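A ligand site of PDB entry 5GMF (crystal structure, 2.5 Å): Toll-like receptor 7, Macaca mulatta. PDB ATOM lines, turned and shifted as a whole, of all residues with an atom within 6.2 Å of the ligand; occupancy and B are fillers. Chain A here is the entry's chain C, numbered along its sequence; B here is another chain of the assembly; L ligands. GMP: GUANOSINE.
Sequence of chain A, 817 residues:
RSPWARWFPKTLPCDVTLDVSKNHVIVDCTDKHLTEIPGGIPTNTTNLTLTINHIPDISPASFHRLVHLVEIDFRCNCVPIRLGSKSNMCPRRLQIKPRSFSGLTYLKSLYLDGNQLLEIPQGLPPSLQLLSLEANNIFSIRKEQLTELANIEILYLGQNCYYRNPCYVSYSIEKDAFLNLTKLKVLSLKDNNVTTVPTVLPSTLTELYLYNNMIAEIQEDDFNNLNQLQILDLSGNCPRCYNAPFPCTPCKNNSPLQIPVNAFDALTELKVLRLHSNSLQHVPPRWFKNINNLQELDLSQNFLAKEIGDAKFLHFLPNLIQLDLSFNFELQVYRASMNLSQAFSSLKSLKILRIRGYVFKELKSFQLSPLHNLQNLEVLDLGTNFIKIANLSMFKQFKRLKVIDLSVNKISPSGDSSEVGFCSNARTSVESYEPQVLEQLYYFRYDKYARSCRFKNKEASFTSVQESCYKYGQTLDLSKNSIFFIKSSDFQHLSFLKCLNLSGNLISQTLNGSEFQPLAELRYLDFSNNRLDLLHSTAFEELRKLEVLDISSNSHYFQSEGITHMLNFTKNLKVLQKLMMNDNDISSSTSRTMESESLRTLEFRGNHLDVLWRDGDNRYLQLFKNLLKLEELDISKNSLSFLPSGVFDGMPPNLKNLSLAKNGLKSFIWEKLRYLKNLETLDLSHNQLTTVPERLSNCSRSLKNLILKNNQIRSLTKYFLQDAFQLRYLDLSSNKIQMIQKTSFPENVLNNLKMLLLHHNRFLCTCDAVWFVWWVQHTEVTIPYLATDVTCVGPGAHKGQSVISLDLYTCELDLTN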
ATOM      1  N   SER A 508       7.142  -6.863  20.515  1.00  0.00           N
ATOM      2  CA  SER A 508       6.303  -7.818  21.257  1.00  0.00           C
ATOM      3  C   SER A 508       5.220  -8.439  20.398  1.00  0.00           C
ATOM      4  O   SER A 508       4.247  -8.980  20.878  1.00  0.00           O
ATOM      5  CB  SER A 508       5.686  -7.114  22.455  1.00  0.00           C
ATOM      6  OG  SER A 508       6.688  -6.597  23.317  1.00  0.00           O
ATOM      7  N   THR A 510       3.445 -10.576  17.113  1.00  0.00           N
ATOM      8  CA  THR A 510       3.356 -11.852  16.425  1.00  0.00           C
ATOM      9  C   THR A 510       3.673 -11.683  14.959  1.00  0.00           C
ATOM     10  O   THR A 510       2.804 -11.511  14.120  1.00  0.00           O
ATOM     11  CB  THR A 510       1.980 -12.546  16.576  1.00  0.00           C
ATOM     12  OG1 THR A 510       0.971 -11.736  16.023  1.00  0.00           O
ATOM     13  CG2 THR A 510       1.662 -12.813  18.048  1.00  0.00           C
ATOM     14  N   ASP A 533       7.194 -13.053  19.871  1.00  0.00           N
ATOM     15  CA  ASP A 533       6.050 -13.907  20.098  1.00  0.00           C
ATOM     16  C   ASP A 533       5.884 -14.795  18.886  1.00  0.00           C
ATOM     17  O   ASP A 533       5.212 -14.429  17.953  1.00  0.00           O
ATOM     18  CB  ASP A 533       4.815 -13.054  20.363  1.00  0.00           C
ATOM     19  CG  ASP A 533       3.594 -13.871  20.816  1.00  0.00           C
ATOM     20  OD1 ASP A 533       3.571 -15.122  20.784  1.00  0.00           O
ATOM     21  OD2 ASP A 533       2.595 -13.204  21.181  1.00  0.00           O
ATOM     22  N   LEU A 534       6.436 -15.994  18.953  1.00  0.00           N
ATOM     23  CA  LEU A 534       6.369 -16.938  17.870  1.00  0.00           C
ATOM     24  C   LEU A 534       5.034 -17.703  17.797  1.00  0.00           C
ATOM     25  O   LEU A 534       5.019 -18.928  17.757  1.00  0.00           O
ATOM     26  CB  LEU A 534       7.518 -17.959  17.987  1.00  0.00           C
ATOM     27  CG  LEU A 534       8.817 -17.576  17.354  1.00  0.00           C
ATOM     28  CD1 LEU A 534       9.833 -18.669  17.659  1.00  0.00           C
ATOM     29  CD2 LEU A 534       8.662 -17.413  15.848  1.00  0.00           C
ATOM     30  N   LEU A 535       3.929 -16.989  17.678  1.00  0.00           N
ATOM     31  CA  LEU A 535       2.641 -17.628  17.428  1.00  0.00           C
ATOM     32  C   LEU A 535       2.559 -18.306  16.055  1.00  0.00           C
ATOM     33  O   LEU A 535       2.032 -19.417  15.948  1.00  0.00           O
ATOM     34  CB  LEU A 535       1.524 -16.610  17.547  1.00  0.00           C
ATOM     35  CG  LEU A 535       0.081 -17.074  17.225  1.00  0.00           C
ATOM     36  CD1 LEU A 535      -0.328 -18.265  18.077  1.00  0.00           C
ATOM     37  CD2 LEU A 535      -0.886 -15.910  17.425  1.00  0.00           C
ATOM     38  N   TYR A 557       7.770 -14.241  26.306  1.00  0.00           N
ATOM     39  CA  TYR A 557       6.577 -15.110  26.137  1.00  0.00           C
ATOM     40  C   TYR A 557       6.779 -16.594  26.375  1.00  0.00           C
ATOM     41  O   TYR A 557       5.826 -17.322  26.580  1.00  0.00           O
ATOM     42  CB  TYR A 557       5.938 -14.909  24.782  1.00  0.00           C
ATOM     43  CG  TYR A 557       5.366 -13.506  24.680  1.00  0.00           C
ATOM     44  CD1 TYR A 557       4.249 -13.127  25.432  1.00  0.00           C
ATOM     45  CD2 TYR A 557       5.959 -12.558  23.858  1.00  0.00           C
ATOM     46  CE1 TYR A 557       3.762 -11.838  25.350  1.00  0.00           C
ATOM     47  CE2 TYR A 557       5.472 -11.269  23.776  1.00  0.00           C
ATOM     48  CZ  TYR A 557       4.367 -10.933  24.497  1.00  0.00           C
ATOM     49  OH  TYR A 557       3.929  -9.651  24.367  1.00  0.00           O
ATOM     50  N   GLY A 562       0.829 -21.863  28.814  1.00  0.00           N
ATOM     51  CA  GLY A 562      -0.354 -21.886  27.966  1.00  0.00           C
ATOM     52  C   GLY A 562      -0.276 -21.080  26.673  1.00  0.00           C
ATOM     53  O   GLY A 562      -1.300 -20.919  25.997  1.00  0.00           O
ATOM     54  N   ILE A 563       0.908 -20.586  26.316  1.00  0.00           N
ATOM     55  CA  ILE A 563       1.108 -19.779  25.131  1.00  0.00           C
ATOM     56  C   ILE A 563       1.612 -20.643  24.000  1.00  0.00           C
ATOM     57  O   ILE A 563       2.611 -21.323  24.144  1.00  0.00           O
ATOM     58  CB  ILE A 563       2.085 -18.624  25.380  1.00  0.00           C
ATOM     59  CG1 ILE A 563       1.547 -17.715  26.496  1.00  0.00           C
ATOM     60  CG2 ILE A 563       2.274 -17.807  24.116  1.00  0.00           C
ATOM     61  CD1 ILE A 563       2.324 -16.404  26.744  1.00  0.00           C
ATOM     62  N   THR A 564       0.939 -20.583  22.865  1.00  0.00           N
ATOM     63  CA  THR A 564       1.291 -21.354  21.702  1.00  0.00           C
ATOM     64  C   THR A 564       2.547 -20.720  21.085  1.00  0.00           C
ATOM     65  O   THR A 564       2.573 -19.508  20.882  1.00  0.00           O
ATOM     66  CB  THR A 564       0.145 -21.337  20.714  1.00  0.00           C
ATOM     67  OG1 THR A 564      -0.966 -22.018  21.278  1.00  0.00           O
ATOM     68  CG2 THR A 564       0.489 -22.002  19.378  1.00  0.00           C
ATOM     69  N   HIS A 565       3.553 -21.567  20.825  1.00  0.00           N
ATOM     70  CA  HIS A 565       4.834 -21.193  20.268  1.00  0.00           C
ATOM     71  C   HIS A 565       5.114 -22.157  19.132  1.00  0.00           C
ATOM     72  O   HIS A 565       5.006 -23.381  19.309  1.00  0.00           O
ATOM     73  CB  HIS A 565       5.984 -21.394  21.264  1.00  0.00           C
ATOM     74  CG  HIS A 565       5.818 -20.703  22.568  1.00  0.00           C
ATOM     75  ND1 HIS A 565       5.648 -19.326  22.658  1.00  0.00           N
ATOM     76  CD2 HIS A 565       5.885 -21.163  23.834  1.00  0.00           C
ATOM     77  CE1 HIS A 565       5.555 -18.992  23.931  1.00  0.00           C
ATOM     78  NE2 HIS A 565       5.708 -20.083  24.665  1.00  0.00           N
ATOM     79  N   TYR B 242      -4.398 -29.594  24.103  1.00  0.00           N
ATOM     80  CA  TYR B 242      -3.706 -28.504  23.399  1.00  0.00           C
ATOM     81  C   TYR B 242      -2.657 -27.850  24.305  1.00  0.00           C
ATOM     82  O   TYR B 242      -2.982 -27.411  25.394  1.00  0.00           O
ATOM     83  CB  TYR B 242      -4.713 -27.447  22.904  1.00  0.00           C
ATOM     84  CG  TYR B 242      -4.122 -26.400  21.966  1.00  0.00           C
ATOM     85  CD1 TYR B 242      -3.650 -26.757  20.716  1.00  0.00           C
ATOM     86  CD2 TYR B 242      -4.061 -25.062  22.336  1.00  0.00           C
ATOM     87  CE1 TYR B 242      -3.133 -25.827  19.851  1.00  0.00           C
ATOM     88  CE2 TYR B 242      -3.554 -24.123  21.466  1.00  0.00           C
ATOM     89  CZ  TYR B 242      -3.084 -24.505  20.232  1.00  0.00           C
ATOM     90  OH  TYR B 242      -2.547 -23.567  19.364  1.00  0.00           O
ATOM     91  N   ASN B 243      -1.402 -27.862  23.852  1.00  0.00           N
ATOM     92  CA  ASN B 243      -0.242 -27.413  24.628  1.00  0.00           C
ATOM     93  C   ASN B 243      -0.057 -28.104  25.970  1.00  0.00           C
ATOM     94  O   ASN B 243       0.406 -27.481  26.920  1.00  0.00           O
ATOM     95  CB  ASN B 243      -0.268 -25.889  24.828  1.00  0.00           C
ATOM     96  CG  ASN B 243      -0.032 -25.115  23.545  1.00  0.00           C
ATOM     97  OD1 ASN B 243       0.744 -25.536  22.672  1.00  0.00           O
ATOM     98  ND2 ASN B 243      -0.678 -23.952  23.437  1.00  0.00           N
ATOM     99  N   PHE B 329     -10.601 -21.425  25.993  1.00  0.00           N
ATOM    100  CA  PHE B 329     -10.724 -20.824  24.673  1.00  0.00           C
ATOM    101  C   PHE B 329     -10.977 -21.842  23.581  1.00  0.00           C
ATOM    102  O   PHE B 329     -10.511 -22.964  23.656  1.00  0.00           O
ATOM    103  CB  PHE B 329      -9.512 -19.937  24.344  1.00  0.00           C
ATOM    104  CG  PHE B 329      -8.193 -20.678  24.210  1.00  0.00           C
ATOM    105  CD1 PHE B 329      -7.284 -20.693  25.259  1.00  0.00           C
ATOM    106  CD2 PHE B 329      -7.831 -21.245  23.015  1.00  0.00           C
ATOM    107  CE1 PHE B 329      -6.067 -21.330  25.130  1.00  0.00           C
ATOM    108  CE2 PHE B 329      -6.627 -21.871  22.859  1.00  0.00           C
ATOM    109  CZ  PHE B 329      -5.731 -21.925  23.919  1.00  0.00           C
ATOM    110  N   GLU B 330     -11.690 -21.425  22.539  1.00  0.00           N
ATOM    111  CA  GLU B 330     -11.905 -22.239  21.346  1.00  0.00           C
ATOM    112  C   GLU B 330     -10.598 -22.160  20.576  1.00  0.00           C
ATOM    113  O   GLU B 330     -10.089 -21.074  20.339  1.00  0.00           O
ATOM    114  CB  GLU B 330     -13.067 -21.689  20.474  1.00  0.00           C
ATOM    115  CG  GLU B 330     -14.376 -21.381  21.246  1.00  0.00           C
ATOM    116  CD  GLU B 330     -15.410 -20.565  20.451  1.00  0.00           C
ATOM    117  OE1 GLU B 330     -15.689 -19.388  20.818  1.00  0.00           O
ATOM    118  OE2 GLU B 330     -15.962 -21.129  19.475  1.00  0.00           O
ATOM    119  N   LEU B 331     -10.043 -23.291  20.192  1.00  0.00           N
ATOM    120  CA  LEU B 331      -8.781 -23.291  19.472  1.00  0.00           C
ATOM    121  C   LEU B 331      -8.928 -22.489  18.182  1.00  0.00           C
ATOM    122  O   LEU B 331      -9.977 -22.545  17.524  1.00  0.00           O
ATOM    123  CB  LEU B 331      -8.327 -24.703  19.128  1.00  0.00           C
ATOM    124  CG  LEU B 331      -8.305 -25.801  20.218  1.00  0.00           C
ATOM    125  CD1 LEU B 331      -7.433 -26.966  19.802  1.00  0.00           C
ATOM    126  CD2 LEU B 331      -7.794 -25.251  21.521  1.00  0.00           C
ATOM    127  N   GLN B 332      -7.893 -21.730  17.855  1.00  0.00           N
ATOM    128  CA  GLN B 332      -7.796 -20.969  16.612  1.00  0.00           C
ATOM    129  C   GLN B 332      -8.746 -19.749  16.548  1.00  0.00           C
ATOM    130  O   GLN B 332      -8.861 -19.143  15.494  1.00  0.00           O
ATOM    131  CB  GLN B 332      -8.010 -21.865  15.348  1.00  0.00           C
ATOM    132  CG  GLN B 332      -7.267 -23.203  15.309  1.00  0.00           C
ATOM    133  CD  GLN B 332      -5.779 -23.028  15.591  1.00  0.00           C
ATOM    134  OE1 GLN B 332      -5.164 -22.082  15.099  1.00  0.00           O
ATOM    135  NE2 GLN B 332      -5.192 -23.918  16.406  1.00  0.00           N
ATOM    136  N   VAL B 333      -9.387 -19.371  17.660  1.00  0.00           N
ATOM    137  CA  VAL B 333     -10.321 -18.260  17.691  1.00  0.00           C
ATOM    138  C   VAL B 333      -9.789 -17.200  18.626  1.00  0.00           C
ATOM    139  O   VAL B 333      -9.362 -17.514  19.733  1.00  0.00           O
ATOM    140  CB  VAL B 333     -11.705 -18.680  18.189  1.00  0.00           C
ATOM    141  CG1 VAL B 333     -12.641 -17.479  18.364  1.00  0.00           C
ATOM    142  CG2 VAL B 333     -12.363 -19.660  17.229  1.00  0.00           C
ATOM    143  N   TYR B 334      -9.831 -15.947  18.198  1.00  0.00           N
ATOM    144  CA  TYR B 334      -9.448 -14.813  19.040  1.00  0.00           C
ATOM    145  C   TYR B 334     -10.665 -13.885  19.163  1.00  0.00           C
ATOM    146  O   TYR B 334     -10.825 -12.979  18.371  1.00  0.00           O
ATOM    147  CB  TYR B 334      -8.259 -14.127  18.370  1.00  0.00           C
ATOM    148  CG  TYR B 334      -7.500 -13.077  19.153  1.00  0.00           C
ATOM    149  CD1 TYR B 334      -7.682 -12.901  20.525  1.00  0.00           C
ATOM    150  CD2 TYR B 334      -6.518 -12.295  18.504  1.00  0.00           C
ATOM    151  CE1 TYR B 334      -6.924 -11.943  21.229  1.00  0.00           C
ATOM    152  CE2 TYR B 334      -5.805 -11.328  19.190  1.00  0.00           C
ATOM    153  CZ  TYR B 334      -5.997 -11.166  20.558  1.00  0.00           C
ATOM    154  OH  TYR B 334      -5.270 -10.229  21.260  1.00  0.00           O
ATOM    155  N   VAL B 359      -9.161 -15.607  26.082  1.00  0.00           N
ATOM    156  CA  VAL B 359      -8.450 -15.172  24.846  1.00  0.00           C
ATOM    157  C   VAL B 359      -9.330 -14.193  24.041  1.00  0.00           C
ATOM    158  O   VAL B 359     -10.154 -14.598  23.204  1.00  0.00           O
ATOM    159  CB  VAL B 359      -7.874 -16.349  24.015  1.00  0.00           C
ATOM    160  CG1 VAL B 359      -7.088 -15.842  22.820  1.00  0.00           C
ATOM    161  CG2 VAL B 359      -6.955 -17.196  24.871  1.00  0.00           C
ATOM    162  N   ASN B 385      -4.898 -13.513  28.688  1.00  0.00           N
ATOM    163  CA  ASN B 385      -5.962 -13.378  27.745  1.00  0.00           C
ATOM    164  C   ASN B 385      -5.635 -12.668  26.450  1.00  0.00           C
ATOM    165  O   ASN B 385      -6.560 -12.418  25.659  1.00  0.00           O
ATOM    166  CB  ASN B 385      -7.150 -12.691  28.443  1.00  0.00           C
ATOM    167  CG  ASN B 385      -7.958 -13.671  29.263  1.00  0.00           C
ATOM    168  OD1 ASN B 385      -8.464 -14.651  28.736  1.00  0.00           O
ATOM    169  ND2 ASN B 385      -8.073 -13.409  30.531  1.00  0.00           N
ATOM    170  N   PHE B 386      -4.389 -12.282  26.264  1.00  0.00           N
ATOM    171  CA  PHE B 386      -3.977 -11.476  25.074  1.00  0.00           C
ATOM    172  C   PHE B 386      -4.858 -10.271  24.825  1.00  0.00           C
ATOM    173  O   PHE B 386      -5.176  -9.944  23.675  1.00  0.00           O
ATOM    174  CB  PHE B 386      -3.856 -12.360  23.851  1.00  0.00           C
ATOM    175  CG  PHE B 386      -2.884 -13.492  24.054  1.00  0.00           C
ATOM    176  CD1 PHE B 386      -1.517 -13.271  23.938  1.00  0.00           C
ATOM    177  CD2 PHE B 386      -3.329 -14.739  24.465  1.00  0.00           C
ATOM    178  CE1 PHE B 386      -0.603 -14.296  24.152  1.00  0.00           C
ATOM    179  CE2 PHE B 386      -2.425 -15.752  24.710  1.00  0.00           C
ATOM    180  CZ  PHE B 386      -1.056 -15.532  24.543  1.00  0.00           C
ATOM    181  N   LYS B 388      -5.699  -6.608  24.301  1.00  0.00           N
ATOM    182  CA  LYS B 388      -4.942  -5.468  23.732  1.00  0.00           C
ATOM    183  C   LYS B 388      -5.443  -4.106  24.249  1.00  0.00           C
ATOM    184  O   LYS B 388      -4.680  -3.139  24.305  1.00  0.00           O
ATOM    185  CB  LYS B 388      -4.986  -5.497  22.193  1.00  0.00           C
ATOM    186  CG  LYS B 388      -4.744  -6.865  21.580  1.00  0.00           C
ATOM    187  CD  LYS B 388      -4.691  -6.833  20.066  1.00  0.00           C
ATOM    188  CE  LYS B 388      -3.238  -6.532  19.636  1.00  0.00           C
ATOM    189  NZ  LYS B 388      -2.781  -7.339  18.461  1.00  0.00           N
ATOM    190  N   LYS B 410      -1.631  -8.161  26.536  1.00  0.00           N
ATOM    191  CA  LYS B 410      -0.974  -7.364  25.503  1.00  0.00           C
ATOM    192  C   LYS B 410      -1.442  -5.921  25.547  1.00  0.00           C
ATOM    193  O   LYS B 410      -1.571  -5.255  24.548  1.00  0.00           O
ATOM    194  CB  LYS B 410      -1.181  -8.076  24.138  1.00  0.00           C
ATOM    195  CG  LYS B 410       0.147  -8.587  23.562  1.00  0.00           C
ATOM    196  CD  LYS B 410       0.177 -10.040  23.218  1.00  0.00           C
ATOM    197  CE  LYS B 410       1.577 -10.447  22.733  1.00  0.00           C
ATOM    198  NZ  LYS B 410       1.732 -10.451  21.259  1.00  0.00           N
HETATM  199  O5' GMP L   1      -1.285 -18.547  22.242  1.00  0.00           O
HETATM  200  C5' GMP L   1      -2.335 -19.210  22.934  1.00  0.00           C
HETATM  201  C4' GMP L   1      -3.657 -19.005  22.212  1.00  0.00           C
HETATM  202  O4' GMP L   1      -3.899 -17.615  22.217  1.00  0.00           O
HETATM  203  C3' GMP L   1      -3.585 -19.503  20.803  1.00  0.00           C
HETATM  204  O3' GMP L   1      -4.759 -20.217  20.424  1.00  0.00           O
HETATM  205  C2' GMP L   1      -3.448 -18.220  20.044  1.00  0.00           C
HETATM  206  O2' GMP L   1      -4.036 -18.294  18.756  1.00  0.00           O
HETATM  207  C1' GMP L   1      -4.113 -17.189  20.912  1.00  0.00           C
HETATM  208  N9  GMP L   1      -3.558 -15.849  20.725  1.00  0.00           N
HETATM  209  C8  GMP L   1      -4.287 -14.744  20.433  1.00  0.00           C
HETATM  210  N7  GMP L   1      -3.486 -13.636  20.329  1.00  0.00           N
HETATM  211  C5  GMP L   1      -2.205 -14.060  20.550  1.00  0.00           C
HETATM  212  C6  GMP L   1      -0.828 -13.450  20.614  1.00  0.00           C
HETATM  213  O6  GMP L   1      -0.599 -12.226  20.436  1.00  0.00           O
HETATM  214  N1  GMP L   1       0.180 -14.262  20.895  1.00  0.00           N
HETATM  215  C2  GMP L   1       0.038 -15.568  21.151  1.00  0.00           C
HETATM  216  N2  GMP L   1       1.134 -16.332  21.403  1.00  0.00           N
HETATM  217  N3  GMP L   1      -1.156 -16.163  21.126  1.00  0.00           N
HETATM  218  C4  GMP L   1      -2.282 -15.500  20.840  1.00  0.00           C
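OD2 of Asp 533 sits at hydrogen-bond distance from N1 of the ligand, at 2.7 Å.
N of Thr 564 is in hydrogen-bond range of O5' of the ligand, at 3.1 Å.
NZ of Lys 410 of chain B is in hydrogen-bond range of O6 of the ligand (3.0 Å).
NE2 of His 565 lies close to O of Ile 563 (3.4 Å).
The side-chain hydroxyl (OG1) of Thr 564 is in hydrogen-bond range of the side-chain hydroxyl (OH) of Tyr 242 of chain B.
O of Phe 386 of chain B sits at hydrogen-bond distance from OH of Tyr 334 of chain B (2.4 Å).
The side-chain amino group (NZ) of Lys 410 of chain B lies within hydrogen-bond range of the backbone carbonyl oxygen (O) of Ser 508, at 2.9 Å.
OD2 of Asp 533 is in salt-bridge range of NZ of Lys 410 of chain B (2.9 Å).
The side-chain hydroxyl (OG1) of Thr 564 lies within hydrogen-bond range of the side-chain amide nitrogen (ND2) of Asn 243 of chain B.
N of Val 359 of chain B is in hydrogen-bond range of OD1 of Asn 385 of chain B.
Thr 510 touches the ligand.
Leu 535 touches the ligand (CD1 to C2', 3.7 Å).
Gly 562 touches the ligand (O to C5', 3.7 Å).
Ile 563 touches the ligand (CG2 to N2, 3.3 Å).
Phe 329 of chain B touches the ligand.
CE2 of Tyr 334 of chain B touches N7 of the ligand (3.5 Å).
Val 359 of chain B touches the ligand (CG1 to O4', 3.7 Å).
Phe 386 of chain B touches the ligand.
Hydrophobic or aromatic side chains within 4 Å of the ligand: Leu 535, Ile 563, Phe 329 of chain B, Tyr 334 of chain B, Val 359 of chain B and Phe 386 of chain B.
Within 4 Å of the ligand: Thr 510, Asp 533, Leu 535, Gly 562, Ile 563, Thr 564, Phe 329 of chain B, Tyr 334 of chain B, Val 359 of chain B, Phe 386 of chain B and Lys 410 of chain B.
Along chain A the residues within 4 Å of the ligand span positions 510 to 564.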
